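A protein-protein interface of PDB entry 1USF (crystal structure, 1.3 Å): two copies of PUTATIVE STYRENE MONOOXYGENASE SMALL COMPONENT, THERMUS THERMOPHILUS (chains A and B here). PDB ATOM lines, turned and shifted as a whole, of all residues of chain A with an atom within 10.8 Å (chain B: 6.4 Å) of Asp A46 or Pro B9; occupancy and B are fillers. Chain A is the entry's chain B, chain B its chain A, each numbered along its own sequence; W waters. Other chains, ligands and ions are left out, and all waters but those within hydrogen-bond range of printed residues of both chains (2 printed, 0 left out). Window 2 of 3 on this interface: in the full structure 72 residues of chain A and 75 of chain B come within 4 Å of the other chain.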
ATOM      1  N   GLY A  42      20.488  11.040   8.004  1.00  0.00           N
ATOM      2  CA  GLY A  42      19.882  10.808   9.297  1.00  0.00           C
ATOM      3  C   GLY A  42      18.612  11.637   9.214  1.00  0.00           C
ATOM      4  O   GLY A  42      18.564  12.622   8.475  1.00  0.00           O
ATOM      5  N   LEU A  43      17.569  11.244   9.940  1.00  0.00           N
ATOM      6  CA  LEU A  43      16.316  11.992   9.905  1.00  0.00           C
ATOM      7  C   LEU A  43      15.789  12.351  11.291  1.00  0.00           C
ATOM      8  O   LEU A  43      14.966  13.257  11.429  1.00  0.00           O
ATOM      9  CB  LEU A  43      15.253  11.210   9.131  1.00  0.00           C
ATOM     10  CG  LEU A  43      15.482  11.157   7.618  1.00  0.00           C
ATOM     11  CD1 LEU A  43      14.437  10.258   6.973  1.00  0.00           C
ATOM     12  CD2 LEU A  43      15.413  12.571   7.026  1.00  0.00           C
ATOM     13  N   SER A  44      16.263  11.644  12.309  1.00  0.00           N
ATOM     14  CA  SER A  44      15.843  11.894  13.686  1.00  0.00           C
ATOM     15  C   SER A  44      16.795  11.187  14.632  1.00  0.00           C
ATOM     16  O   SER A  44      17.286  10.104  14.326  1.00  0.00           O
ATOM     17  CB  SER A  44      14.412  11.377  13.912  1.00  0.00           C
ATOM     18  OG  SER A  44      14.016  11.527  15.271  1.00  0.00           O
ATOM     19  N   ALA A  45      17.061  11.798  15.781  1.00  0.00           N
ATOM     20  CA  ALA A  45      17.949  11.190  16.765  1.00  0.00           C
ATOM     21  C   ALA A  45      17.123  10.414  17.786  1.00  0.00           C
ATOM     22  O   ALA A  45      17.475   9.302  18.168  1.00  0.00           O
ATOM     23  CB  ALA A  45      18.780  12.261  17.469  1.00  0.00           C
ATOM     24  N   ASP A  46      16.021  11.010  18.219  1.00  0.00           N
ATOM     25  CA  ASP A  46      15.139  10.380  19.195  1.00  0.00           C
ATOM     26  C   ASP A  46      13.698  10.449  18.697  1.00  0.00           C
ATOM     27  O   ASP A  46      13.044  11.484  18.804  1.00  0.00           O
ATOM     28  CB  ASP A  46      15.267  11.092  20.546  1.00  0.00           C
ATOM     29  CG  ASP A  46      14.391  10.474  21.620  1.00  0.00           C
ATOM     30  OD1 ASP A  46      13.882   9.353  21.411  1.00  0.00           O
ATOM     31  OD2 ASP A  46      14.224  11.111  22.681  1.00  0.00           O
ATOM     32  N   PRO A  47      13.182   9.339  18.139  1.00  0.00           N
ATOM     33  CA  PRO A  47      13.864   8.055  17.959  1.00  0.00           C
ATOM     34  C   PRO A  47      14.859   8.104  16.805  1.00  0.00           C
ATOM     35  O   PRO A  47      14.804   9.002  15.963  1.00  0.00           O
ATOM     36  CB  PRO A  47      12.713   7.101  17.679  1.00  0.00           C
ATOM     37  CG  PRO A  47      11.800   7.952  16.860  1.00  0.00           C
ATOM     38  CD  PRO A  47      11.811   9.281  17.599  1.00  0.00           C
ATOM     39  N   PRO A  48      15.786   7.136  16.751  1.00  0.00           N
ATOM     40  CA  PRO A  48      16.781   7.104  15.676  1.00  0.00           C
ATOM     41  C   PRO A  48      16.164   6.663  14.350  1.00  0.00           C
ATOM     42  O   PRO A  48      15.789   5.500  14.186  1.00  0.00           O
ATOM     43  CB  PRO A  48      17.822   6.121  16.203  1.00  0.00           C
ATOM     44  CG  PRO A  48      16.987   5.155  16.993  1.00  0.00           C
ATOM     45  CD  PRO A  48      16.034   6.066  17.735  1.00  0.00           C
ATOM     46  N   LEU A  49      16.041   7.603  13.417  1.00  0.00           N
ATOM     47  CA  LEU A  49      15.474   7.318  12.103  1.00  0.00           C
ATOM     48  C   LEU A  49      16.512   7.640  11.039  1.00  0.00           C
ATOM     49  O   LEU A  49      17.221   8.641  11.134  1.00  0.00           O
ATOM     50  CB  LEU A  49      14.212   8.148  11.864  1.00  0.00           C
ATOM     51  CG  LEU A  49      13.106   8.008  12.912  1.00  0.00           C
ATOM     52  CD1 LEU A  49      11.918   8.881  12.523  1.00  0.00           C
ATOM     53  CD2 LEU A  49      12.692   6.545  13.035  1.00  0.00           C
ATOM     54  N   PHE A  50      16.582   6.786  10.025  1.00  0.00           N
ATOM     55  CA  PHE A  50      17.543   6.925   8.939  1.00  0.00           C
ATOM     56  C   PHE A  50      16.809   6.703   7.624  1.00  0.00           C
ATOM     57  O   PHE A  50      16.007   5.780   7.510  1.00  0.00           O
ATOM     58  CB  PHE A  50      18.633   5.868   9.120  1.00  0.00           C
ATOM     59  CG  PHE A  50      19.735   5.941   8.107  1.00  0.00           C
ATOM     60  CD1 PHE A  50      20.698   6.940   8.176  1.00  0.00           C
ATOM     61  CD2 PHE A  50      19.814   5.004   7.087  1.00  0.00           C
ATOM     62  CE1 PHE A  50      21.732   7.008   7.241  1.00  0.00           C
ATOM     63  CE2 PHE A  50      20.843   5.062   6.144  1.00  0.00           C
ATOM     64  CZ  PHE A  50      21.802   6.066   6.223  1.00  0.00           C
ATOM     65  N   TYR A 118      23.109  -0.727  10.384  1.00  0.00           N
ATOM     66  CA  TYR A 118      21.851  -0.582  11.103  1.00  0.00           C
ATOM     67  C   TYR A 118      20.854  -1.593  10.572  1.00  0.00           C
ATOM     68  O   TYR A 118      20.831  -1.889   9.374  1.00  0.00           O
ATOM     69  CB  TYR A 118      21.220   0.795  10.865  1.00  0.00           C
ATOM     70  CG  TYR A 118      21.966   1.989  11.398  1.00  0.00           C
ATOM     71  CD1 TYR A 118      21.839   3.228  10.771  1.00  0.00           C
ATOM     72  CD2 TYR A 118      22.761   1.904  12.541  1.00  0.00           C
ATOM     73  CE1 TYR A 118      22.482   4.351  11.262  1.00  0.00           C
ATOM     74  CE2 TYR A 118      23.410   3.027  13.046  1.00  0.00           C
ATOM     75  CZ  TYR A 118      23.266   4.246  12.397  1.00  0.00           C
ATOM     76  OH  TYR A 118      23.910   5.361  12.869  1.00  0.00           O
ATOM     77  N   LEU A 123       9.253   2.530   8.456  1.00  0.00           N
ATOM     78  CA  LEU A 123       8.228   3.320   9.128  1.00  0.00           C
ATOM     79  C   LEU A 123       7.278   3.973   8.126  1.00  0.00           C
ATOM     80  O   LEU A 123       6.059   3.813   8.214  1.00  0.00           O
ATOM     81  CB  LEU A 123       8.898   4.400   9.982  1.00  0.00           C
ATOM     82  CG  LEU A 123       8.013   5.340  10.803  1.00  0.00           C
ATOM     83  CD1 LEU A 123       7.254   4.548  11.852  1.00  0.00           C
ATOM     84  CD2 LEU A 123       8.880   6.400  11.463  1.00  0.00           C
ATOM     85  N   GLY A 136      13.429   4.568   7.759  1.00  0.00           N
ATOM     86  CA  GLY A 136      13.513   3.430   8.647  1.00  0.00           C
ATOM     87  C   GLY A 136      13.880   3.784  10.070  1.00  0.00           C
ATOM     88  O   GLY A 136      14.570   4.771  10.334  1.00  0.00           O
ATOM     89  N   ARG A 137      13.394   2.972  10.998  1.00  0.00           N
ATOM     90  CA  ARG A 137      13.691   3.163  12.404  1.00  0.00           C
ATOM     91  C   ARG A 137      14.798   2.180  12.749  1.00  0.00           C
ATOM     92  O   ARG A 137      14.695   0.992  12.447  1.00  0.00           O
ATOM     93  CB  ARG A 137      12.452   2.877  13.252  1.00  0.00           C
ATOM     94  CG  ARG A 137      12.661   3.096  14.737  1.00  0.00           C
ATOM     95  CD  ARG A 137      11.332   3.095  15.476  1.00  0.00           C
ATOM     96  NE  ARG A 137      11.465   3.628  16.828  1.00  0.00           N
ATOM     97  CZ  ARG A 137      10.438   3.944  17.611  1.00  0.00           C
ATOM     98  NH1 ARG A 137       9.195   3.782  17.178  1.00  0.00           N
ATOM     99  NH2 ARG A 137      10.653   4.426  18.827  1.00  0.00           N
ATOM    100  N   VAL A 138      15.863   2.677  13.362  1.00  0.00           N
ATOM    101  CA  VAL A 138      16.972   1.817  13.744  1.00  0.00           C
ATOM    102  C   VAL A 138      16.544   0.940  14.918  1.00  0.00           C
ATOM    103  O   VAL A 138      16.172   1.450  15.981  1.00  0.00           O
ATOM    104  CB  VAL A 138      18.205   2.644  14.156  1.00  0.00           C
ATOM    105  CG1 VAL A 138      19.341   1.718  14.567  1.00  0.00           C
ATOM    106  CG2 VAL A 138      18.631   3.547  13.001  1.00  0.00           C
ATOM    107  N   VAL A 139      16.584  -0.375  14.723  1.00  0.00           N
ATOM    108  CA  VAL A 139      16.196  -1.300  15.786  1.00  0.00           C
ATOM    109  C   VAL A 139      17.370  -2.115  16.320  1.00  0.00           C
ATOM    110  O   VAL A 139      17.280  -2.733  17.380  1.00  0.00           O
ATOM    111  CB  VAL A 139      15.067  -2.253  15.324  1.00  0.00           C
ATOM    112  CG1 VAL A 139      13.804  -1.456  15.025  1.00  0.00           C
ATOM    113  CG2 VAL A 139      15.506  -3.039  14.102  1.00  0.00           C
ATOM    114  N   ALA A 140      18.475  -2.119  15.585  1.00  0.00           N
ATOM    115  CA  ALA A 140      19.670  -2.824  16.018  1.00  0.00           C
ATOM    116  C   ALA A 140      20.876  -2.168  15.370  1.00  0.00           C
ATOM    117  O   ALA A 140      20.783  -1.656  14.251  1.00  0.00           O
ATOM    118  CB  ALA A 140      19.596  -4.298  15.644  1.00  0.00           C
ATOM    119  N   VAL A 141      21.999  -2.195  16.080  1.00  0.00           N
ATOM    120  CA  VAL A 141      23.245  -1.588  15.619  1.00  0.00           C
ATOM    121  C   VAL A 141      24.414  -2.568  15.655  1.00  0.00           C
ATOM    122  O   VAL A 141      24.587  -3.310  16.622  1.00  0.00           O
ATOM    123  CB  VAL A 141      23.617  -0.366  16.499  1.00  0.00           C
ATOM    124  CG1 VAL A 141      24.856   0.321  15.951  1.00  0.00           C
ATOM    125  CG2 VAL A 141      22.450   0.601  16.561  1.00  0.00           C
ATOM    126  N   GLU A 143      28.688  -2.849  15.032  1.00  0.00           N
ATOM    127  CA  GLU A 143      29.913  -2.059  14.977  1.00  0.00           C
ATOM    128  C   GLU A 143      31.155  -2.940  14.994  1.00  0.00           C
ATOM    129  O   GLU A 143      31.234  -3.899  15.764  1.00  0.00           O
ATOM    130  CB  GLU A 143      29.988  -1.108  16.175  1.00  0.00           C
ATOM    131  CG  GLU A 143      28.722  -0.322  16.456  1.00  0.00           C
ATOM    132  CD  GLU A 143      28.872   0.599  17.653  1.00  0.00           C
ATOM    133  OE1 GLU A 143      29.491   0.180  18.655  1.00  0.00           O
ATOM    134  OE2 GLU A 143      28.367   1.737  17.602  1.00  0.00           O
ATOM    135  N   GLN B   7      17.555   0.932  21.999  1.00  0.00           N
ATOM    136  CA  GLN B   7      16.677   1.080  23.157  1.00  0.00           C
ATOM    137  C   GLN B   7      16.227   2.527  23.308  1.00  0.00           C
ATOM    138  O   GLN B   7      15.599   2.905  24.302  1.00  0.00           O
ATOM    139  CB  GLN B   7      17.430   0.618  24.409  1.00  0.00           C
ATOM    140  CG  GLN B   7      17.813  -0.857  24.369  1.00  0.00           C
ATOM    141  CD  GLN B   7      19.093  -1.170  25.127  1.00  0.00           C
ATOM    142  OE1 GLN B   7      19.202  -0.916  26.329  1.00  0.00           O
ATOM    143  NE2 GLN B   7      20.071  -1.733  24.423  1.00  0.00           N
ATOM    144  N   GLY B   8      16.550   3.324  22.297  1.00  0.00           N
ATOM    145  CA  GLY B   8      16.210   4.733  22.288  1.00  0.00           C
ATOM    146  C   GLY B   8      17.274   5.415  21.454  1.00  0.00           C
ATOM    147  O   GLY B   8      17.858   4.775  20.580  1.00  0.00           O
ATOM    148  N   PRO B   9      17.563   6.701  21.693  1.00  0.00           N
ATOM    149  CA  PRO B   9      18.593   7.384  20.903  1.00  0.00           C
ATOM    150  C   PRO B   9      19.914   6.643  21.079  1.00  0.00           C
ATOM    151  O   PRO B   9      20.195   6.123  22.159  1.00  0.00           O
ATOM    152  CB  PRO B   9      18.649   8.777  21.526  1.00  0.00           C
ATOM    153  CG  PRO B   9      17.304   8.939  22.173  1.00  0.00           C
ATOM    154  CD  PRO B   9      17.029   7.584  22.742  1.00  0.00           C
ATOM    155  N   LEU B  10      20.724   6.584  20.028  1.00  0.00           N
ATOM    156  CA  LEU B  10      22.006   5.897  20.117  1.00  0.00           C
ATOM    157  C   LEU B  10      23.014   6.738  20.896  1.00  0.00           C
ATOM    158  O   LEU B  10      22.922   7.964  20.917  1.00  0.00           O
ATOM    159  CB  LEU B  10      22.553   5.615  18.715  1.00  0.00           C
ATOM    160  CG  LEU B  10      21.614   4.893  17.749  1.00  0.00           C
ATOM    161  CD1 LEU B  10      22.386   4.515  16.493  1.00  0.00           C
ATOM    162  CD2 LEU B  10      21.040   3.643  18.401  1.00  0.00           C
ATOM    163  N   PRO B  11      23.986   6.088  21.563  1.00  0.00           N
ATOM    164  CA  PRO B  11      24.983   6.848  22.324  1.00  0.00           C
ATOM    165  C   PRO B  11      25.645   7.873  21.410  1.00  0.00           C
ATOM    166  O   PRO B  11      25.977   8.982  21.826  1.00  0.00           O
ATOM    167  CB  PRO B  11      25.954   5.769  22.791  1.00  0.00           C
ATOM    168  CG  PRO B  11      25.056   4.583  22.970  1.00  0.00           C
ATOM    169  CD  PRO B  11      24.180   4.639  21.737  1.00  0.00           C
ATOM    170  N   GLY B  12      25.819   7.470  20.157  1.00  0.00           N
ATOM    171  CA  GLY B  12      26.407   8.316  19.136  1.00  0.00           C
ATOM    172  C   GLY B  12      25.790   7.872  17.824  1.00  0.00           C
ATOM    173  O   GLY B  12      25.962   6.727  17.418  1.00  0.00           O
ATOM    174  N   GLY B 129      10.190  12.000  13.471  1.00  0.00           N
ATOM    175  CA  GLY B 129      10.807  12.049  14.780  1.00  0.00           C
ATOM    176  C   GLY B 129      11.072  13.476  15.227  1.00  0.00           C
ATOM    177  O   GLY B 129      10.197  14.338  15.106  1.00  0.00           O
ATOM    178  N   ASP B 130      12.285  13.739  15.707  1.00  0.00           N
ATOM    179  CA  ASP B 130      12.625  15.066  16.211  1.00  0.00           C
ATOM    180  C   ASP B 130      13.148  16.109  15.220  1.00  0.00           C
ATOM    181  O   ASP B 130      13.618  17.165  15.638  1.00  0.00           O
ATOM    182  CB  ASP B 130      13.599  14.957  17.398  1.00  0.00           C
ATOM    183  CG  ASP B 130      14.932  14.325  17.025  1.00  0.00           C
ATOM    184  OD1 ASP B 130      15.312  14.366  15.838  1.00  0.00           O
ATOM    185  OD2 ASP B 130      15.613  13.805  17.938  1.00  0.00           O
HETATM  186  O   HOH W   1      10.491  12.462  18.366  1.00  0.00           O
HETATM  187  O   HOH W   2      20.069   8.495  17.943  1.00  0.00           O
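No position is printed for both chains. Of the 10 pairs that touch across the chains among the printed residues, none has its exchanged pair printed and touching as well.
Printed residues of chain B that touch a printed residue of chain A: Gly B8, Pro B9, Leu B10, Gly B129 and Asp B130. Among the printed residues, no Asp or Glu carboxylate lies within 4 Å of a Lys or Arg side-chain nitrogen of the other chain.
Ser A44 touches Gly B129. Ala A45 touches Pro B9. CG of Pro B9 touches CG of Asp A46 (3.3 Å). Gly B8 touches Pro A48 (O to CD, 3.6 Å). N of Gly B129 touches CD1 of Leu A49, 3.7 Å away. Tyr A118 touches Leu B10 (CE2 to CD1, 3.9 Å). Val A141 touches Leu B10 (CG2 to CD2, 3.8 Å).
The backbone NH of Asp B130 lies within hydrogen-bond range of the side-chain hydroxyl of Ser A44, 2.8 Å away. OD1 of Asp B130 sits at hydrogen-bond distance from N of Ala A45, at 3.1 Å. The backbone NH of Asp A46 sits at hydrogen-bond distance from the side-chain carboxylate of Asp B130, at 2.8 Å.
N of Leu A43 is in hydrogen-bond range of O of Leu A49. OG of Ser A44 lies within hydrogen-bond range of O of Pro A47 (2.7 Å). The backbone carbonyl oxygen (O) of Ser A44 sits at hydrogen-bond distance from the backbone NH (N) of Leu A49, at 2.9 Å. The backbone NH (N) of Val A138 is in hydrogen-bond range of the backbone carbonyl oxygen (O) of Pro A48 (2.9 Å).
Water W2 bridges O of Ala A45 and N of Leu B10. Water W1 bridges O of Asp A46 and N of Asp B130.
Of chain B, only Pro B9 (3.3 Å) and Asp B130 (2.8 Å) come within 4 Å of Asp A46. Of chain A, only Ala A45 and Asp A46 come within 4 Å of Pro B9. Gly B8 touches one residue of chain A. Printed residues of chain B within 4 Å of Ser A44: Gly B129 (3.3 Å) and Asp B130 (2.8 Å). Of the printed residues of chain B, Tyr A118 touches Leu B10 (3.9 Å). Gly B12 touches none of the printed residues of chain A. Arg A137 touches none of the printed residues of chain B. The nearest printed residue of chain B that does not touch Pro A48 is Leu B10 (4.3 Å).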
